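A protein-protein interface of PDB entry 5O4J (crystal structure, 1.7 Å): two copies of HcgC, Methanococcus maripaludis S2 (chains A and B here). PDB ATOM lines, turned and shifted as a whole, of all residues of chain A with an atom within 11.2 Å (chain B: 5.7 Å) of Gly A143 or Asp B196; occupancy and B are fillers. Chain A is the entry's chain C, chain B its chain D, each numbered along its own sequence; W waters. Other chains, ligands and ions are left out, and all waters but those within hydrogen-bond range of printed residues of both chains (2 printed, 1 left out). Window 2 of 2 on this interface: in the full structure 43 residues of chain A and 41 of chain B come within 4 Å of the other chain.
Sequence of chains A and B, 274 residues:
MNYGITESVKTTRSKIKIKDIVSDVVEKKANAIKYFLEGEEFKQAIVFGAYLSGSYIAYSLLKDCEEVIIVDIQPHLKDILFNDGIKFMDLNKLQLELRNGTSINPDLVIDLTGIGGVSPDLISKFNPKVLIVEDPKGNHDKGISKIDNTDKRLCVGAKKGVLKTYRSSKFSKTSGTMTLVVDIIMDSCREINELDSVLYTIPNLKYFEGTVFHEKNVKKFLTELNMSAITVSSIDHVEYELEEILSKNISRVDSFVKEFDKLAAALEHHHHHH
Of chain B, only Asp B196 comes within 4 Å of Gly A143.
Of the printed residues of chain B, Ile A144 touches Val B198.
Of the printed residues of chain B, Ile A147 touches Ile B235.
Printed residues of chain B within 4 Å of Lys A173: Asn B193 (2.8 Å), Leu B195 (2.8 Å) and Val B198 (2.9 Å).
Of the printed residues of chain A, Asn B193 touches Lys A173 (2.8 Å).
Of the printed residues of chain A, Leu B195 touches Asp A141 and Lys A173.
Of the printed residues of chain A, Asp B196 touches Asp A141, Lys A142 and Gly A143.
Ser B197 touches one residue of chain A.
No residue of chain A comes within 4 Å of Asp B236.
The nearest residue of chain B that does not touch Gly A143 is Ser B197 (4.2 Å).
The nearest residue of chain A that does not touch Asp B196 is Lys A173 (4.6 Å).
The nearest printed residue of chain A that does not touch Asn B193 is Phe A171 (5.0 Å).
Among the printed residues, merely in contact across the chains: Asp A141 with Asp B196 (3.5 Å), Ile A147 with Ile B235 (3.6 Å), Ile A144 with Val B198 (3.7 Å) and Asp A141 with Leu B195 (3.8 Å).
Hydrophobic or aromatic side chains of chain A within 4 Å of the printed part of chain B: Ile A144 and Ile A147.
Hydrophobic or aromatic side chains of chain B within 4 Å of the printed part of chain A: Val B198 and Ile B235.
The backbone carbonyl oxygen (O) of Lys A173 is in hydrogen-bond range of the backbone NH (N) of Gly A138, at 3.2 Å.
OD1 of Asp A141 sits at hydrogen-bond distance from N of Ile A144 (2.8 Å).
The side-chain hydroxyl of Ser A145 sits at hydrogen-bond distance from the backbone carbonyl oxygen of Asp A141, 3.3 Å away.
The side-chain amino group (NZ) of Lys A173 is in salt-bridge range of the side-chain carboxylate (OD2) of Asp A141, at 2.8 Å.
N of Ile B235 lies within hydrogen-bond range of O of Ser B197 (2.9 Å).
OG of Ser B197 is in hydrogen-bond range of N of Asp B236 (3.0 Å).
The backbone NH (N) of Ser B197 sits at hydrogen-bond distance from the side-chain carboxylate (OD2) of Asp A141 (2.9 Å).
The backbone NH (N) of Lys A142 is in hydrogen-bond range of the side-chain carboxylate (OD1) of Asp B196 (3.4 Å).
The side-chain carboxylate (OD1) of Asp B196 sits at hydrogen-bond distance from the backbone NH (N) of Gly A143.
O of Asn B193 is in hydrogen-bond range of NZ of Lys A173 (2.8 Å).
The side-chain amino group of Lys A173 lies within hydrogen-bond range of the backbone carbonyl oxygen of Leu B195 (2.8 Å).
NZ of Lys A173 is in hydrogen-bond range of O of Val B198 (2.9 Å).
No position is printed for both chains.
Water W1 lies within hydrogen-bond range of OD2 of Asp B196 (2.5 Å), NZ of Lys A146 (2.7 Å) and N of Gly A143 (3.4 Å).
Water W2 bridges N of Lys A173 (2.9 Å) and ND2 of Asn B193 (3.1 Å).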
ATOM      1  N   ILE A 115      -4.131 -23.124 -12.356  1.00  0.00           N
ATOM      2  CA  ILE A 115      -3.930 -24.531 -12.689  1.00  0.00           C
ATOM      3  C   ILE A 115      -2.525 -24.977 -12.316  1.00  0.00           C
ATOM      4  O   ILE A 115      -1.530 -24.339 -12.685  1.00  0.00           O
ATOM      5  CB  ILE A 115      -4.214 -24.762 -14.182  1.00  0.00           C
ATOM      6  CG1 ILE A 115      -5.690 -24.493 -14.478  1.00  0.00           C
ATOM      7  CG2 ILE A 115      -3.838 -26.184 -14.592  1.00  0.00           C
ATOM      8  CD1 ILE A 115      -5.995 -24.316 -15.958  1.00  0.00           C
ATOM      9  N   GLY A 116      -2.439 -26.109 -11.616  1.00  0.00           N
ATOM     10  CA  GLY A 116      -1.167 -26.668 -11.202  1.00  0.00           C
ATOM     11  C   GLY A 116      -0.410 -25.825 -10.206  1.00  0.00           C
ATOM     12  O   GLY A 116       0.807 -25.991 -10.061  1.00  0.00           O
ATOM     13  N   PRO A 136      -9.230 -20.419 -12.065  1.00  0.00           N
ATOM     14  CA  PRO A 136      -8.704 -20.394 -13.434  1.00  0.00           C
ATOM     15  C   PRO A 136      -9.710 -20.842 -14.464  1.00  0.00           C
ATOM     16  O   PRO A 136      -9.486 -20.615 -15.659  1.00  0.00           O
ATOM     17  CB  PRO A 136      -7.517 -21.363 -13.370  1.00  0.00           C
ATOM     18  CG  PRO A 136      -7.946 -22.360 -12.352  1.00  0.00           C
ATOM     19  CD  PRO A 136      -8.731 -21.592 -11.319  1.00  0.00           C
ATOM     20  N   LYS A 137     -10.796 -21.487 -14.050  1.00  0.00           N
ATOM     21  CA  LYS A 137     -11.783 -21.953 -15.014  1.00  0.00           C
ATOM     22  C   LYS A 137     -12.453 -20.766 -15.691  1.00  0.00           C
ATOM     23  O   LYS A 137     -12.854 -19.800 -15.031  1.00  0.00           O
ATOM     24  CB  LYS A 137     -12.837 -22.824 -14.338  1.00  0.00           C
ATOM     25  CG  LYS A 137     -12.295 -24.091 -13.711  1.00  0.00           C
ATOM     26  CD  LYS A 137     -13.410 -25.006 -13.222  1.00  0.00           C
ATOM     27  CE  LYS A 137     -14.351 -24.333 -12.236  1.00  0.00           C
ATOM     28  NZ  LYS A 137     -13.639 -23.829 -11.036  1.00  0.00           N
ATOM     29  N   GLY A 138     -12.566 -20.844 -17.012  1.00  0.00           N
ATOM     30  CA  GLY A 138     -13.374 -19.904 -17.755  1.00  0.00           C
ATOM     31  C   GLY A 138     -14.722 -20.532 -18.013  1.00  0.00           C
ATOM     32  O   GLY A 138     -15.389 -21.001 -17.082  1.00  0.00           O
ATOM     33  N   ASN A 139     -15.124 -20.572 -19.272  1.00  0.00           N
ATOM     34  CA  ASN A 139     -16.340 -21.266 -19.643  1.00  0.00           C
ATOM     35  C   ASN A 139     -16.038 -22.762 -19.711  1.00  0.00           C
ATOM     36  O   ASN A 139     -14.932 -23.207 -19.390  1.00  0.00           O
ATOM     37  CB  ASN A 139     -16.865 -20.661 -20.935  1.00  0.00           C
ATOM     38  CG  ASN A 139     -16.980 -19.147 -20.831  1.00  0.00           C
ATOM     39  OD1 ASN A 139     -16.433 -18.410 -21.658  1.00  0.00           O
ATOM     40  ND2 ASN A 139     -17.651 -18.672 -19.781  1.00  0.00           N
ATOM     41  N   HIS A 140     -17.024 -23.575 -20.081  1.00  0.00           N
ATOM     42  CA  HIS A 140     -16.944 -24.980 -19.715  1.00  0.00           C
ATOM     43  C   HIS A 140     -15.987 -25.766 -20.600  1.00  0.00           C
ATOM     44  O   HIS A 140     -16.064 -25.720 -21.834  1.00  0.00           O
ATOM     45  CB  HIS A 140     -18.310 -25.657 -19.735  1.00  0.00           C
ATOM     46  CG  HIS A 140     -18.290 -26.999 -19.067  1.00  0.00           C
ATOM     47  ND1 HIS A 140     -17.850 -27.168 -17.768  1.00  0.00           N
ATOM     48  CD2 HIS A 140     -18.623 -28.229 -19.518  1.00  0.00           C
ATOM     49  CE1 HIS A 140     -17.929 -28.448 -17.447  1.00  0.00           C
ATOM     50  NE2 HIS A 140     -18.399 -29.111 -18.488  1.00  0.00           N
ATOM     51  N   ASP A 141     -15.129 -26.547 -19.947  1.00  0.00           N
ATOM     52  CA  ASP A 141     -14.220 -27.469 -20.613  1.00  0.00           C
ATOM     53  C   ASP A 141     -13.975 -28.612 -19.639  1.00  0.00           C
ATOM     54  O   ASP A 141     -13.512 -28.384 -18.519  1.00  0.00           O
ATOM     55  CB  ASP A 141     -12.900 -26.778 -20.999  1.00  0.00           C
ATOM     56  CG  ASP A 141     -11.886 -27.732 -21.645  1.00  0.00           C
ATOM     57  OD1 ASP A 141     -11.115 -28.403 -20.907  1.00  0.00           O
ATOM     58  OD2 ASP A 141     -11.846 -27.790 -22.899  1.00  0.00           O
ATOM     59  N   LYS A 142     -14.308 -29.835 -20.049  1.00  0.00           N
ATOM     60  CA  LYS A 142     -14.218 -30.956 -19.119  1.00  0.00           C
ATOM     61  C   LYS A 142     -12.791 -31.190 -18.653  1.00  0.00           C
ATOM     62  O   LYS A 142     -12.558 -31.471 -17.474  1.00  0.00           O
ATOM     63  CB  LYS A 142     -14.766 -32.220 -19.775  1.00  0.00           C
ATOM     64  CG  LYS A 142     -16.239 -32.160 -20.059  1.00  0.00           C
ATOM     65  CD  LYS A 142     -16.714 -33.507 -20.621  1.00  0.00           C
ATOM     66  CE  LYS A 142     -18.173 -33.459 -21.040  1.00  0.00           C
ATOM     67  NZ  LYS A 142     -18.588 -34.680 -21.776  1.00  0.00           N
ATOM     68  N   GLY A 143     -11.824 -31.106 -19.567  1.00  0.00           N
ATOM     69  CA  GLY A 143     -10.440 -31.364 -19.196  1.00  0.00           C
ATOM     70  C   GLY A 143      -9.913 -30.381 -18.168  1.00  0.00           C
ATOM     71  O   GLY A 143      -9.194 -30.759 -17.240  1.00  0.00           O
ATOM     72  N   ILE A 144     -10.253 -29.103 -18.323  1.00  0.00           N
ATOM     73  CA  ILE A 144      -9.812 -28.095 -17.369  1.00  0.00           C
ATOM     74  C   ILE A 144     -10.549 -28.253 -16.043  1.00  0.00           C
ATOM     75  O   ILE A 144      -9.959 -28.084 -14.970  1.00  0.00           O
ATOM     76  CB  ILE A 144     -10.004 -26.691 -17.968  1.00  0.00           C
ATOM     77  CG1 ILE A 144      -9.036 -26.512 -19.142  1.00  0.00           C
ATOM     78  CG2 ILE A 144      -9.802 -25.619 -16.908  1.00  0.00           C
ATOM     79  CD1 ILE A 144      -9.350 -25.334 -20.027  1.00  0.00           C
ATOM     80  N   SER A 145     -11.851 -28.558 -16.089  1.00  0.00           N
ATOM     81  CA  SER A 145     -12.592 -28.780 -14.850  1.00  0.00           C
ATOM     82  C   SER A 145     -11.964 -29.902 -14.035  1.00  0.00           C
ATOM     83  O   SER A 145     -11.885 -29.815 -12.802  1.00  0.00           O
ATOM     84  CB  SER A 145     -14.054 -29.104 -15.153  1.00  0.00           C
ATOM     85  OG  SER A 145     -14.767 -27.938 -15.517  1.00  0.00           O
ATOM     86  N   LYS A 146     -11.491 -30.947 -14.715  1.00  0.00           N
ATOM     87  CA  LYS A 146     -10.937 -32.121 -14.046  1.00  0.00           C
ATOM     88  C   LYS A 146      -9.698 -31.772 -13.240  1.00  0.00           C
ATOM     89  O   LYS A 146      -9.481 -32.324 -12.157  1.00  0.00           O
ATOM     90  CB  LYS A 146     -10.577 -33.189 -15.083  1.00  0.00           C
ATOM     91  CG  LYS A 146     -11.551 -34.338 -15.224  1.00  0.00           C
ATOM     92  CD  LYS A 146     -11.004 -35.322 -16.253  1.00  0.00           C
ATOM     93  CE  LYS A 146     -11.988 -35.598 -17.372  1.00  0.00           C
ATOM     94  NZ  LYS A 146     -11.324 -36.290 -18.517  1.00  0.00           N
ATOM     95  N   ILE A 147      -8.850 -30.887 -13.772  1.00  0.00           N
ATOM     96  CA  ILE A 147      -7.583 -30.560 -13.126  1.00  0.00           C
ATOM     97  C   ILE A 147      -7.722 -29.418 -12.127  1.00  0.00           C
ATOM     98  O   ILE A 147      -6.796 -29.178 -11.334  1.00  0.00           O
ATOM     99  CB  ILE A 147      -6.518 -30.242 -14.197  1.00  0.00           C
ATOM    100  CG1 ILE A 147      -5.107 -30.300 -13.592  1.00  0.00           C
ATOM    101  CG2 ILE A 147      -6.754 -28.872 -14.828  1.00  0.00           C
ATOM    102  CD1 ILE A 147      -4.033 -30.680 -14.590  1.00  0.00           C
ATOM    103  N   ASP A 148      -8.845 -28.711 -12.134  1.00  0.00           N
ATOM    104  CA  ASP A 148      -9.048 -27.599 -11.224  1.00  0.00           C
ATOM    105  C   ASP A 148      -9.352 -28.094  -9.814  1.00  0.00           C
ATOM    106  O   ASP A 148     -10.066 -29.082  -9.627  1.00  0.00           O
ATOM    107  CB  ASP A 148     -10.192 -26.720 -11.722  1.00  0.00           C
ATOM    108  CG  ASP A 148     -10.532 -25.633 -10.744  1.00  0.00           C
ATOM    109  OD1 ASP A 148      -9.703 -24.714 -10.585  1.00  0.00           O
ATOM    110  OD2 ASP A 148     -11.621 -25.700 -10.136  1.00  0.00           O
ATOM    111  N   ASN A 149      -8.806 -27.401  -8.813  1.00  0.00           N
ATOM    112  CA  ASN A 149      -9.121 -27.717  -7.427  1.00  0.00           C
ATOM    113  C   ASN A 149      -9.302 -26.435  -6.623  1.00  0.00           C
ATOM    114  O   ASN A 149      -8.959 -26.365  -5.435  1.00  0.00           O
ATOM    115  CB  ASN A 149      -8.051 -28.625  -6.822  1.00  0.00           C
ATOM    116  CG  ASN A 149      -6.706 -27.937  -6.673  1.00  0.00           C
ATOM    117  OD1 ASN A 149      -6.460 -26.894  -7.265  1.00  0.00           O
ATOM    118  ND2 ASN A 149      -5.816 -28.540  -5.881  1.00  0.00           N
ATOM    119  N   PHE A 171     -16.764 -16.931 -25.577  1.00  0.00           N
ATOM    120  CA  PHE A 171     -16.193 -18.122 -24.958  1.00  0.00           C
ATOM    121  C   PHE A 171     -14.685 -17.964 -24.759  1.00  0.00           C
ATOM    122  O   PHE A 171     -13.956 -17.642 -25.705  1.00  0.00           O
ATOM    123  CB  PHE A 171     -16.472 -19.360 -25.822  1.00  0.00           C
ATOM    124  CG  PHE A 171     -16.108 -20.641 -25.151  1.00  0.00           C
ATOM    125  CD1 PHE A 171     -14.803 -21.097 -25.173  1.00  0.00           C
ATOM    126  CD2 PHE A 171     -17.058 -21.372 -24.461  1.00  0.00           C
ATOM    127  CE1 PHE A 171     -14.453 -22.257 -24.525  1.00  0.00           C
ATOM    128  CE2 PHE A 171     -16.722 -22.532 -23.818  1.00  0.00           C
ATOM    129  CZ  PHE A 171     -15.412 -22.974 -23.842  1.00  0.00           C
ATOM    130  N   LYS A 173     -11.499 -20.272 -22.483  1.00  0.00           N
ATOM    131  CA  LYS A 173     -11.277 -21.521 -21.756  1.00  0.00           C
ATOM    132  C   LYS A 173     -10.819 -21.307 -20.326  1.00  0.00           C
ATOM    133  O   LYS A 173     -11.015 -22.194 -19.486  1.00  0.00           O
ATOM    134  CB  LYS A 173     -10.239 -22.382 -22.479  1.00  0.00           C
ATOM    135  CG  LYS A 173     -10.744 -23.028 -23.756  1.00  0.00           C
ATOM    136  CD  LYS A 173     -11.695 -24.170 -23.427  1.00  0.00           C
ATOM    137  CE  LYS A 173     -11.970 -25.078 -24.620  1.00  0.00           C
ATOM    138  NZ  LYS A 173     -10.896 -26.058 -24.846  1.00  0.00           N
ATOM    139  N   THR A 174     -10.144 -20.196 -20.052  1.00  0.00           N
ATOM    140  CA  THR A 174      -9.689 -19.885 -18.708  1.00  0.00           C
ATOM    141  C   THR A 174      -9.931 -18.408 -18.446  1.00  0.00           C
ATOM    142  O   THR A 174     -10.265 -17.620 -19.339  1.00  0.00           O
ATOM    143  CB  THR A 174      -8.193 -20.219 -18.470  1.00  0.00           C
ATOM    144  OG1 THR A 174      -7.358 -19.149 -18.940  1.00  0.00           O
ATOM    145  CG2 THR A 174      -7.785 -21.538 -19.123  1.00  0.00           C
ATOM    146  N   ASN B 193      -8.901 -24.498 -30.564  1.00  0.00           N
ATOM    147  CA  ASN B 193      -9.222 -24.003 -29.231  1.00  0.00           C
ATOM    148  C   ASN B 193     -10.377 -24.776 -28.608  1.00  0.00           C
ATOM    149  O   ASN B 193     -10.449 -24.904 -27.381  1.00  0.00           O
ATOM    150  CB  ASN B 193      -9.552 -22.519 -29.274  1.00  0.00           C
ATOM    151  CG  ASN B 193      -9.225 -21.830 -27.975  1.00  0.00           C
ATOM    152  OD1 ASN B 193      -8.066 -21.766 -27.582  1.00  0.00           O
ATOM    153  ND2 ASN B 193     -10.243 -21.317 -27.296  1.00  0.00           N
ATOM    154  N   GLU B 194     -11.281 -25.300 -29.432  1.00  0.00           N
ATOM    155  CA  GLU B 194     -12.421 -26.044 -28.927  1.00  0.00           C
ATOM    156  C   GLU B 194     -12.083 -27.487 -28.596  1.00  0.00           C
ATOM    157  O   GLU B 194     -12.930 -28.186 -28.032  1.00  0.00           O
ATOM    158  CB  GLU B 194     -13.566 -25.974 -29.950  1.00  0.00           C
ATOM    159  CG  GLU B 194     -14.118 -24.551 -30.075  1.00  0.00           C
ATOM    160  CD  GLU B 194     -15.339 -24.445 -30.976  1.00  0.00           C
ATOM    161  OE1 GLU B 194     -15.619 -25.416 -31.689  1.00  0.00           O
ATOM    162  OE2 GLU B 194     -16.018 -23.393 -30.947  1.00  0.00           O
ATOM    163  N   LEU B 195     -10.878 -27.960 -28.897  1.00  0.00           N
ATOM    164  CA  LEU B 195     -10.505 -29.295 -28.437  1.00  0.00           C
ATOM    165  C   LEU B 195     -10.535 -29.342 -26.920  1.00  0.00           C
ATOM    166  O   LEU B 195     -10.152 -28.379 -26.246  1.00  0.00           O
ATOM    167  CB  LEU B 195      -9.120 -29.673 -28.934  1.00  0.00           C
ATOM    168  CG  LEU B 195      -8.976 -29.843 -30.440  1.00  0.00           C
ATOM    169  CD1 LEU B 195      -7.494 -29.944 -30.759  1.00  0.00           C
ATOM    170  CD2 LEU B 195      -9.735 -31.069 -30.945  1.00  0.00           C
ATOM    171  N   ASP B 196     -11.000 -30.466 -26.378  1.00  0.00           N
ATOM    172  CA  ASP B 196     -11.041 -30.625 -24.930  1.00  0.00           C
ATOM    173  C   ASP B 196      -9.656 -30.413 -24.332  1.00  0.00           C
ATOM    174  O   ASP B 196      -8.660 -30.956 -24.824  1.00  0.00           O
ATOM    175  CB  ASP B 196     -11.552 -32.017 -24.555  1.00  0.00           C
ATOM    176  CG  ASP B 196     -11.647 -32.213 -23.042  1.00  0.00           C
ATOM    177  OD1 ASP B 196     -12.301 -31.388 -22.366  1.00  0.00           O
ATOM    178  OD2 ASP B 196     -11.054 -33.180 -22.530  1.00  0.00           O
ATOM    179  N   SER B 197      -9.609 -29.638 -23.251  1.00  0.00           N
ATOM    180  CA  SER B 197      -8.448 -29.392 -22.403  1.00  0.00           C
ATOM    181  C   SER B 197      -7.541 -28.278 -22.930  1.00  0.00           C
ATOM    182  O   SER B 197      -6.585 -27.925 -22.245  1.00  0.00           O
ATOM    183  CB  SER B 197      -7.586 -30.653 -22.191  1.00  0.00           C
ATOM    184  OG  SER B 197      -6.624 -30.798 -23.232  1.00  0.00           O
ATOM    185  N   VAL B 198      -7.788 -27.717 -24.116  1.00  0.00           N
ATOM    186  CA  VAL B 198      -6.992 -26.590 -24.589  1.00  0.00           C
ATOM    187  C   VAL B 198      -7.347 -25.354 -23.782  1.00  0.00           C
ATOM    188  O   VAL B 198      -8.530 -25.028 -23.608  1.00  0.00           O
ATOM    189  CB  VAL B 198      -7.219 -26.349 -26.084  1.00  0.00           C
ATOM    190  CG1 VAL B 198      -6.572 -25.032 -26.532  1.00  0.00           C
ATOM    191  CG2 VAL B 198      -6.684 -27.516 -26.887  1.00  0.00           C
ATOM    192  N   SER B 234      -2.406 -26.734 -23.410  1.00  0.00           N
ATOM    193  CA  SER B 234      -3.486 -27.667 -23.111  1.00  0.00           C
ATOM    194  C   SER B 234      -3.114 -28.555 -21.925  1.00  0.00           C
ATOM    195  O   SER B 234      -1.941 -28.690 -21.569  1.00  0.00           O
ATOM    196  CB  SER B 234      -3.822 -28.546 -24.333  1.00  0.00           C
ATOM    197  OG  SER B 234      -2.752 -29.418 -24.678  1.00  0.00           O
ATOM    198  N   ILE B 235      -4.136 -29.167 -21.314  1.00  0.00           N
ATOM    199  CA  ILE B 235      -3.890 -30.154 -20.263  1.00  0.00           C
ATOM    200  C   ILE B 235      -3.518 -31.499 -20.872  1.00  0.00           C
ATOM    201  O   ILE B 235      -2.647 -32.205 -20.350  1.00  0.00           O
ATOM    202  CB  ILE B 235      -5.105 -30.300 -19.328  1.00  0.00           C
ATOM    203  CG1 ILE B 235      -5.598 -28.942 -18.832  1.00  0.00           C
ATOM    204  CG2 ILE B 235      -4.742 -31.189 -18.129  1.00  0.00           C
ATOM    205  CD1 ILE B 235      -4.558 -28.143 -18.067  1.00  0.00           C
ATOM    206  N   ASP B 236      -4.181 -31.888 -21.957  1.00  0.00           N
ATOM    207  CA  ASP B 236      -3.978 -33.194 -22.569  1.00  0.00           C
ATOM    208  C   ASP B 236      -3.230 -33.062 -23.890  1.00  0.00           C
ATOM    209  O   ASP B 236      -3.100 -31.978 -24.467  1.00  0.00           O
ATOM    210  CB  ASP B 236      -5.308 -33.912 -22.823  1.00  0.00           C
ATOM    211  CG  ASP B 236      -6.119 -34.122 -21.561  1.00  0.00           C
ATOM    212  OD1 ASP B 236      -5.525 -34.236 -20.473  1.00  0.00           O
ATOM    213  OD2 ASP B 236      -7.361 -34.229 -21.670  1.00  0.00           O
ATOM    214  N   VAL B 238      -2.588 -33.010 -27.690  1.00  0.00           N
ATOM    215  CA  VAL B 238      -3.393 -32.583 -28.832  1.00  0.00           C
ATOM    216  C   VAL B 238      -2.595 -32.654 -30.128  1.00  0.00           C
ATOM    217  O   VAL B 238      -3.025 -32.121 -31.155  1.00  0.00           O
ATOM    218  CB  VAL B 238      -3.931 -31.157 -28.619  1.00  0.00           C
ATOM    219  CG1 VAL B 238      -4.923 -31.137 -27.468  1.00  0.00           C
ATOM    220  CG2 VAL B 238      -2.777 -30.200 -28.356  1.00  0.00           C
HETATM  221  O   HOH W   1     -11.755 -34.424 -20.432  1.00  0.00           O
HETATM  222  O   HOH W   2      -9.604 -19.841 -24.654  1.00  0.00           O
